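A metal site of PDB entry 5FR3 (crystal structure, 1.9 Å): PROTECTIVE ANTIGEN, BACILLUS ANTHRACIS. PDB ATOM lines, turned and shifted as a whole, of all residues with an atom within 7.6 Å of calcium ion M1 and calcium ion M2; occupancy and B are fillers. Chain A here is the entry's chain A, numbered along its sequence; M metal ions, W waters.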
ATOM      1  N   TYR A   9       9.017  19.088 -13.054  1.00  0.00           N
ATOM      2  CA  TYR A   9       8.691  20.432 -12.598  1.00  0.00           C
ATOM      3  C   TYR A   9       7.185  20.485 -12.384  1.00  0.00           C
ATOM      4  O   TYR A   9       6.429  20.260 -13.324  1.00  0.00           O
ATOM      5  CB  TYR A   9       9.096  21.462 -13.654  1.00  0.00           C
ATOM      6  CG  TYR A   9      10.593  21.551 -13.863  1.00  0.00           C
ATOM      7  CD1 TYR A   9      11.258  20.663 -14.704  1.00  0.00           C
ATOM      8  CD2 TYR A   9      11.350  22.527 -13.222  1.00  0.00           C
ATOM      9  CE1 TYR A   9      12.624  20.738 -14.890  1.00  0.00           C
ATOM     10  CE2 TYR A   9      12.718  22.609 -13.415  1.00  0.00           C
ATOM     11  CZ  TYR A   9      13.349  21.714 -14.243  1.00  0.00           C
ATOM     12  OH  TYR A   9      14.707  21.796 -14.439  1.00  0.00           O
ATOM     13  N   PRO A 163      12.559  28.103 -18.249  1.00  0.00           N
ATOM     14  CA  PRO A 163      13.688  29.015 -18.458  1.00  0.00           C
ATOM     15  C   PRO A 163      14.824  28.589 -17.550  1.00  0.00           C
ATOM     16  O   PRO A 163      14.662  28.590 -16.326  1.00  0.00           O
ATOM     17  CB  PRO A 163      13.129  30.376 -18.019  1.00  0.00           C
ATOM     18  CG  PRO A 163      11.639  30.238 -18.111  1.00  0.00           C
ATOM     19  CD  PRO A 163      11.362  28.812 -17.751  1.00  0.00           C
ATOM     20  N   ASP A 164      15.941  28.189 -18.150  1.00  0.00           N
ATOM     21  CA  ASP A 164      17.087  27.693 -17.397  1.00  0.00           C
ATOM     22  C   ASP A 164      18.334  28.026 -18.204  1.00  0.00           C
ATOM     23  O   ASP A 164      18.977  27.139 -18.772  1.00  0.00           O
ATOM     24  CB  ASP A 164      16.955  26.188 -17.163  1.00  0.00           C
ATOM     25  CG  ASP A 164      18.108  25.630 -16.324  1.00  0.00           C
ATOM     26  OD1 ASP A 164      18.833  26.416 -15.694  1.00  0.00           O
ATOM     27  OD2 ASP A 164      18.275  24.396 -16.297  1.00  0.00           O
ATOM     28  N   ARG A 165      18.671  29.307 -18.218  1.00  0.00           N
ATOM     29  CA  ARG A 165      19.730  29.842 -19.080  1.00  0.00           C
ATOM     30  C   ARG A 165      21.067  29.133 -18.902  1.00  0.00           C
ATOM     31  O   ARG A 165      21.819  28.981 -19.866  1.00  0.00           O
ATOM     32  CB  ARG A 165      19.911  31.351 -18.846  1.00  0.00           C
ATOM     33  CG  ARG A 165      18.757  32.203 -19.348  1.00  0.00           C
ATOM     34  CD  ARG A 165      19.124  33.690 -19.380  1.00  0.00           C
ATOM     35  NE  ARG A 165      19.283  34.251 -18.042  1.00  0.00           N
ATOM     36  CZ  ARG A 165      18.278  34.735 -17.312  1.00  0.00           C
ATOM     37  NH1 ARG A 165      17.041  34.716 -17.800  1.00  0.00           N
ATOM     38  NH2 ARG A 165      18.494  35.240 -16.115  1.00  0.00           N
ATOM     39  N   ASP A 166      21.376  28.695 -17.690  1.00  0.00           N
ATOM     40  CA  ASP A 166      22.688  28.103 -17.448  1.00  0.00           C
ATOM     41  C   ASP A 166      22.685  26.572 -17.422  1.00  0.00           C
ATOM     42  O   ASP A 166      23.725  25.955 -17.210  1.00  0.00           O
ATOM     43  CB  ASP A 166      23.326  28.664 -16.156  1.00  0.00           C
ATOM     44  CG  ASP A 166      22.474  28.428 -14.923  1.00  0.00           C
ATOM     45  OD1 ASP A 166      21.505  27.650 -14.995  1.00  0.00           O
ATOM     46  OD2 ASP A 166      22.802  28.996 -13.869  1.00  0.00           O
ATOM     47  N   ASN A 167      21.519  25.979 -17.633  1.00  0.00           N
ATOM     48  CA  ASN A 167      21.387  24.527 -17.741  1.00  0.00           C
ATOM     49  C   ASN A 167      21.771  23.760 -16.481  1.00  0.00           C
ATOM     50  O   ASN A 167      22.180  22.602 -16.576  1.00  0.00           O
ATOM     51  CB  ASN A 167      22.185  23.983 -18.939  1.00  0.00           C
ATOM     52  CG  ASN A 167      21.597  22.697 -19.498  1.00  0.00           C
ATOM     53  OD1 ASN A 167      20.390  22.577 -19.675  1.00  0.00           O
ATOM     54  ND2 ASN A 167      22.460  21.716 -19.770  1.00  0.00           N
ATOM     55  N   ASP A 168      21.655  24.380 -15.309  1.00  0.00           N
ATOM     56  CA  ASP A 168      21.892  23.637 -14.080  1.00  0.00           C
ATOM     57  C   ASP A 168      20.652  22.867 -13.601  1.00  0.00           C
ATOM     58  O   ASP A 168      20.763  21.908 -12.842  1.00  0.00           O
ATOM     59  CB  ASP A 168      22.507  24.504 -12.955  1.00  0.00           C
ATOM     60  CG  ASP A 168      21.643  25.684 -12.549  1.00  0.00           C
ATOM     61  OD1 ASP A 168      20.432  25.742 -12.894  1.00  0.00           O
ATOM     62  OD2 ASP A 168      22.180  26.558 -11.826  1.00  0.00           O
ATOM     63  N   GLY A 169      19.487  23.273 -14.092  1.00  0.00           N
ATOM     64  CA  GLY A 169      18.248  22.594 -13.726  1.00  0.00           C
ATOM     65  C   GLY A 169      17.300  23.463 -12.911  1.00  0.00           C
ATOM     66  O   GLY A 169      16.098  23.196 -12.851  1.00  0.00           O
ATOM     67  N   ILE A 170      17.849  24.482 -12.265  1.00  0.00           N
ATOM     68  CA  ILE A 170      17.024  25.379 -11.445  1.00  0.00           C
ATOM     69  C   ILE A 170      16.497  26.503 -12.337  1.00  0.00           C
ATOM     70  O   ILE A 170      17.271  27.157 -13.020  1.00  0.00           O
ATOM     71  CB  ILE A 170      17.820  25.967 -10.279  1.00  0.00           C
ATOM     72  CG1 ILE A 170      18.664  24.902  -9.599  1.00  0.00           C
ATOM     73  CG2 ILE A 170      16.881  26.628  -9.281  1.00  0.00           C
ATOM     74  CD1 ILE A 170      19.565  25.421  -8.481  1.00  0.00           C
ATOM     75  N   PRO A 171      15.175  26.714 -12.338  1.00  0.00           N
ATOM     76  CA  PRO A 171      14.582  27.758 -13.185  1.00  0.00           C
ATOM     77  C   PRO A 171      15.178  29.128 -12.883  1.00  0.00           C
ATOM     78  O   PRO A 171      15.544  29.378 -11.717  1.00  0.00           O
ATOM     79  CB  PRO A 171      13.102  27.723 -12.801  1.00  0.00           C
ATOM     80  CG  PRO A 171      12.870  26.306 -12.340  1.00  0.00           C
ATOM     81  CD  PRO A 171      14.146  25.918 -11.642  1.00  0.00           C
ATOM     82  N   ASP A 172      15.301  29.993 -13.900  1.00  0.00           N
ATOM     83  CA  ASP A 172      15.889  31.320 -13.727  1.00  0.00           C
ATOM     84  C   ASP A 172      15.257  32.070 -12.554  1.00  0.00           C
ATOM     85  O   ASP A 172      15.950  32.625 -11.702  1.00  0.00           O
ATOM     86  CB  ASP A 172      15.704  32.185 -14.987  1.00  0.00           C
ATOM     87  CG  ASP A 172      16.384  31.607 -16.211  1.00  0.00           C
ATOM     88  OD1 ASP A 172      17.212  30.691 -16.078  1.00  0.00           O
ATOM     89  OD2 ASP A 172      16.078  32.097 -17.317  1.00  0.00           O
ATOM     90  N   SER A 173      13.924  32.081 -12.523  1.00  0.00           N
ATOM     91  CA  SER A 173      13.176  32.848 -11.535  1.00  0.00           C
ATOM     92  C   SER A 173      13.454  32.419 -10.089  1.00  0.00           C
ATOM     93  O   SER A 173      13.519  33.251  -9.194  1.00  0.00           O
ATOM     94  CB  SER A 173      11.680  32.778 -11.831  1.00  0.00           C
ATOM     95  OG  SER A 173      11.225  31.435 -11.844  1.00  0.00           O
ATOM     96  N   GLU A 175      16.292  30.917  -8.918  1.00  0.00           N
ATOM     97  CA  GLU A 175      17.657  31.281  -8.540  1.00  0.00           C
ATOM     98  C   GLU A 175      17.728  32.747  -8.125  1.00  0.00           C
ATOM     99  O   GLU A 175      18.398  33.105  -7.165  1.00  0.00           O
ATOM    100  CB  GLU A 175      18.634  31.003  -9.691  1.00  0.00           C
ATOM    101  CG  GLU A 175      18.789  29.534 -10.060  1.00  0.00           C
ATOM    102  CD  GLU A 175      20.124  29.216 -10.736  1.00  0.00           C
ATOM    103  OE1 GLU A 175      21.163  29.283 -10.050  1.00  0.00           O
ATOM    104  OE2 GLU A 175      20.127  28.873 -11.932  1.00  0.00           O
ATOM    105  N   TYR A 179      15.160  30.190  -3.313  1.00  0.00           N
ATOM    106  CA  TYR A 179      14.619  28.831  -3.277  1.00  0.00           C
ATOM    107  C   TYR A 179      15.154  28.081  -2.078  1.00  0.00           C
ATOM    108  O   TYR A 179      16.064  28.551  -1.385  1.00  0.00           O
ATOM    109  CB  TYR A 179      14.953  28.074  -4.574  1.00  0.00           C
ATOM    110  CG  TYR A 179      16.432  27.956  -4.886  1.00  0.00           C
ATOM    111  CD1 TYR A 179      17.108  28.984  -5.525  1.00  0.00           C
ATOM    112  CD2 TYR A 179      17.146  26.804  -4.575  1.00  0.00           C
ATOM    113  CE1 TYR A 179      18.453  28.874  -5.836  1.00  0.00           C
ATOM    114  CE2 TYR A 179      18.497  26.693  -4.870  1.00  0.00           C
ATOM    115  CZ  TYR A 179      19.131  27.735  -5.506  1.00  0.00           C
ATOM    116  OH  TYR A 179      20.474  27.618  -5.810  1.00  0.00           O
ATOM    117  N   SER A 208      21.091  32.153  -6.225  1.00  0.00           N
ATOM    118  CA  SER A 208      22.270  31.842  -7.015  1.00  0.00           C
ATOM    119  C   SER A 208      22.145  32.541  -8.356  1.00  0.00           C
ATOM    120  O   SER A 208      21.090  33.100  -8.670  1.00  0.00           O
ATOM    121  CB  SER A 208      22.397  30.336  -7.203  1.00  0.00           C
ATOM    122  OG  SER A 208      21.189  29.763  -7.681  1.00  0.00           O
ATOM    123  N   SER A 209      23.216  32.527  -9.146  1.00  0.00           N
ATOM    124  CA  SER A 209      23.159  33.133 -10.480  1.00  0.00           C
ATOM    125  C   SER A 209      22.482  32.218 -11.492  1.00  0.00           C
ATOM    126  O   SER A 209      22.857  31.063 -11.654  1.00  0.00           O
ATOM    127  CB  SER A 209      24.553  33.493 -10.982  1.00  0.00           C
ATOM    128  OG  SER A 209      24.460  34.014 -12.300  1.00  0.00           O
ATOM    129  N   PRO A 210      21.468  32.740 -12.193  1.00  0.00           N
ATOM    130  CA  PRO A 210      20.806  31.968 -13.252  1.00  0.00           C
ATOM    131  C   PRO A 210      21.651  31.880 -14.518  1.00  0.00           C
ATOM    132  O   PRO A 210      21.225  31.266 -15.484  1.00  0.00           O
ATOM    133  CB  PRO A 210      19.542  32.803 -13.543  1.00  0.00           C
ATOM    134  CG  PRO A 210      19.939  34.199 -13.191  1.00  0.00           C
ATOM    135  CD  PRO A 210      20.800  34.048 -11.970  1.00  0.00           C
ATOM    136  N   GLU A 211      22.829  32.498 -14.508  1.00  0.00           N
ATOM    137  CA  GLU A 211      23.699  32.525 -15.665  1.00  0.00           C
ATOM    138  C   GLU A 211      24.964  31.721 -15.417  1.00  0.00           C
ATOM    139  O   GLU A 211      25.774  31.502 -16.331  1.00  0.00           O
ATOM    140  CB  GLU A 211      24.082  33.963 -15.996  1.00  0.00           C
ATOM    141  CG  GLU A 211      22.922  34.930 -15.967  1.00  0.00           C
ATOM    142  CD  GLU A 211      22.458  35.292 -17.341  1.00  0.00           C
ATOM    143  OE1 GLU A 211      22.593  34.453 -18.249  1.00  0.00           O
ATOM    144  OE2 GLU A 211      21.956  36.429 -17.515  1.00  0.00           O
ATOM    145  N   LYS A 212      25.152  31.296 -14.178  1.00  0.00           N
ATOM    146  CA  LYS A 212      26.324  30.507 -13.814  1.00  0.00           C
ATOM    147  C   LYS A 212      25.902  29.120 -13.374  1.00  0.00           C
ATOM    148  O   LYS A 212      25.199  28.973 -12.382  1.00  0.00           O
ATOM    149  CB  LYS A 212      27.124  31.204 -12.692  1.00  0.00           C
ATOM    150  CG  LYS A 212      27.758  32.526 -13.116  1.00  0.00           C
ATOM    151  CD  LYS A 212      28.498  33.207 -11.966  1.00  0.00           C
ATOM    152  CE  LYS A 212      29.772  32.453 -11.595  1.00  0.00           C
ATOM    153  NZ  LYS A 212      30.772  32.498 -12.695  1.00  0.00           N
ATOM    154  N   TRP A 213      26.325  28.123 -14.131  1.00  0.00           N
ATOM    155  CA  TRP A 213      26.024  26.729 -13.834  1.00  0.00           C
ATOM    156  C   TRP A 213      26.477  26.406 -12.416  1.00  0.00           C
ATOM    157  O   TRP A 213      25.758  25.775 -11.629  1.00  0.00           O
ATOM    158  CB  TRP A 213      26.728  25.843 -14.862  1.00  0.00           C
ATOM    159  CG  TRP A 213      26.614  24.368 -14.651  1.00  0.00           C
ATOM    160  CD1 TRP A 213      25.599  23.543 -15.053  1.00  0.00           C
ATOM    161  CD2 TRP A 213      27.580  23.524 -14.023  1.00  0.00           C
ATOM    162  NE1 TRP A 213      25.872  22.249 -14.692  1.00  0.00           N
ATOM    163  CE2 TRP A 213      27.091  22.204 -14.066  1.00  0.00           C
ATOM    164  CE3 TRP A 213      28.830  23.764 -13.418  1.00  0.00           C
ATOM    165  CZ2 TRP A 213      27.797  21.133 -13.527  1.00  0.00           C
ATOM    166  CZ3 TRP A 213      29.519  22.700 -12.890  1.00  0.00           C
ATOM    167  CH2 TRP A 213      29.013  21.402 -12.945  1.00  0.00           C
ATOM    168  N   SER A 214      27.670  26.880 -12.086  1.00  0.00           N
ATOM    169  CA  SER A 214      28.136  26.927 -10.691  1.00  0.00           C
ATOM    170  C   SER A 214      28.383  28.380 -10.317  1.00  0.00           C
ATOM    171  O   SER A 214      29.287  29.013 -10.864  1.00  0.00           O
ATOM    172  CB  SER A 214      29.418  26.119 -10.504  1.00  0.00           C
ATOM    173  OG  SER A 214      29.952  26.340  -9.198  1.00  0.00           O
ATOM    174  N   THR A 215      27.605  28.902  -9.386  1.00  0.00           N
ATOM    175  CA  THR A 215      27.719  30.313  -9.021  1.00  0.00           C
ATOM    176  C   THR A 215      29.068  30.657  -8.392  1.00  0.00           C
ATOM    177  O   THR A 215      29.585  31.748  -8.587  1.00  0.00           O
ATOM    178  CB  THR A 215      26.557  30.747  -8.132  1.00  0.00           C
ATOM    179  OG1 THR A 215      25.337  30.520  -8.852  1.00  0.00           O
ATOM    180  CG2 THR A 215      26.657  32.223  -7.789  1.00  0.00           C
ATOM    181  N   SER A 221      27.541  21.980  -9.844  1.00  0.00           N
ATOM    182  CA  SER A 221      26.424  22.868 -10.217  1.00  0.00           C
ATOM    183  C   SER A 221      25.609  23.312  -8.999  1.00  0.00           C
ATOM    184  O   SER A 221      25.627  22.656  -7.950  1.00  0.00           O
ATOM    185  CB  SER A 221      25.505  22.209 -11.237  1.00  0.00           C
ATOM    186  OG  SER A 221      24.360  21.631 -10.636  1.00  0.00           O
ATOM    187  N   ASP A 222      24.914  24.434  -9.152  1.00  0.00           N
ATOM    188  CA  ASP A 222      24.075  24.942  -8.070  1.00  0.00           C
ATOM    189  C   ASP A 222      23.023  23.901  -7.693  1.00  0.00           C
ATOM    190  O   ASP A 222      22.688  23.729  -6.531  1.00  0.00           O
ATOM    191  CB  ASP A 222      23.388  26.228  -8.512  1.00  0.00           C
ATOM    192  CG  ASP A 222      24.360  27.356  -8.781  1.00  0.00           C
ATOM    193  OD1 ASP A 222      25.471  27.343  -8.212  1.00  0.00           O
ATOM    194  OD2 ASP A 222      24.003  28.275  -9.550  1.00  0.00           O
ATOM    195  N   PHE A 223      22.525  23.197  -8.705  1.00  0.00           N
ATOM    196  CA  PHE A 223      21.504  22.172  -8.517  1.00  0.00           C
ATOM    197  C   PHE A 223      22.107  20.919  -7.875  1.00  0.00           C
ATOM    198  O   PHE A 223      21.511  20.337  -6.965  1.00  0.00           O
ATOM    199  CB  PHE A 223      20.876  21.854  -9.867  1.00  0.00           C
ATOM    200  CG  PHE A 223      19.820  20.780  -9.824  1.00  0.00           C
ATOM    201  CD1 PHE A 223      18.556  21.051  -9.336  1.00  0.00           C
ATOM    202  CD2 PHE A 223      20.092  19.508 -10.305  1.00  0.00           C
ATOM    203  CE1 PHE A 223      17.580  20.056  -9.318  1.00  0.00           C
ATOM    204  CE2 PHE A 223      19.130  18.514 -10.298  1.00  0.00           C
ATOM    205  CZ  PHE A 223      17.870  18.790  -9.787  1.00  0.00           C
ATOM    206  N   PRO A 241      25.391  27.164  -2.745  1.00  0.00           N
ATOM    207  CA  PRO A 241      25.817  27.598  -4.075  1.00  0.00           C
ATOM    208  C   PRO A 241      26.713  28.839  -4.051  1.00  0.00           C
ATOM    209  O   PRO A 241      27.387  29.099  -5.044  1.00  0.00           O
ATOM    210  CB  PRO A 241      24.479  27.916  -4.778  1.00  0.00           C
ATOM    211  CG  PRO A 241      23.490  27.056  -4.082  1.00  0.00           C
ATOM    212  CD  PRO A 241      23.931  27.030  -2.638  1.00  0.00           C
HETATM  213 CA    CA M   1      22.939  28.781 -11.614  1.00  0.00          CA
HETATM  214 CA    CA M   2      19.435  27.634 -13.800  1.00  0.00          CA
HETATM  215  O   HOH W   1      19.241  29.665 -14.873  1.00  0.00           O
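The backbone NH of Asp 166 sits close to the backbone carbonyl oxygen of Pro 210 (3.4 Å). The side-chain hydroxyl of Ser 209 sits at hydrogen-bond distance from the backbone NH of Lys 212, 3.4 Å away. The side-chain hydroxyl (OG1) of Thr 215 is in hydrogen-bond range of the backbone NH (N) of Ser 209 (2.9 Å). OG of Ser 209 lies close to N of Glu 211 (3.1 Å). N of Asn 167 sits close to OD1 of Asp 164 (3.3 Å). N of Ser 208 sits at hydrogen-bond distance from O of Glu 175 (3.0 Å). The side-chain carboxylate (OD1) of Asp 222 lies within hydrogen-bond range of the backbone NH (N) of Thr 215, 2.9 Å away. N of Asp 222 sits at hydrogen-bond distance from O of Trp 213.
Calcium ion M1 is bound by OD2 of Asp 166 (2.3 Å). Calcium ion M1 is bound by O of Ser 209 (2.3 Å). Calcium ion M1 is bound by OD2 of Asp 168 (2.4 Å). Calcium ion M1 is bound by the side-chain carboxylate (OD2) of Asp 222 (2.4 Å). Calcium ion M1 is bound by O of Lys 212 (2.4 Å). Calcium ion M1 is bound by OE1 of Glu 175, 2.4 Å away. Calcium ion M1 is bound by the side-chain carboxylate (OE2) of Glu 175 (2.8 Å). Calcium ion M1 has seven donor atoms within binding distance.
Within 4 Å of calcium ion M1: Asp 166, Asp 168, Glu 175, Ser 209, Lys 212 and Asp 222.
Water W1 lies within hydrogen-bond range of the side-chain carboxylate of Asp 172, the backbone carbonyl oxygen of Pro 210 and the backbone NH of Arg 165.
Of the 26 residues printed, 5 come within 4 Å of calcium ion M2. The nearest printed residue that does not touch calcium ion M2 is Gly 169 (4.4 Å).
Calcium ion M2 is bound by water W1, 2.3 Å away. The side-chain carboxylate (OD1) of Asp 168 binds calcium ion M2, at 2.3 Å. Calcium ion M2 is bound by OD1 of Asp 164, 2.3 Å away. OE2 of Glu 175 is bound to calcium ion M2 (2.3 Å). O of Ile 170 is bound to calcium ion M2, 2.3 Å away. The side-chain carboxylate (OD1) of Asp 166 binds calcium ion M2 (2.4 Å).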
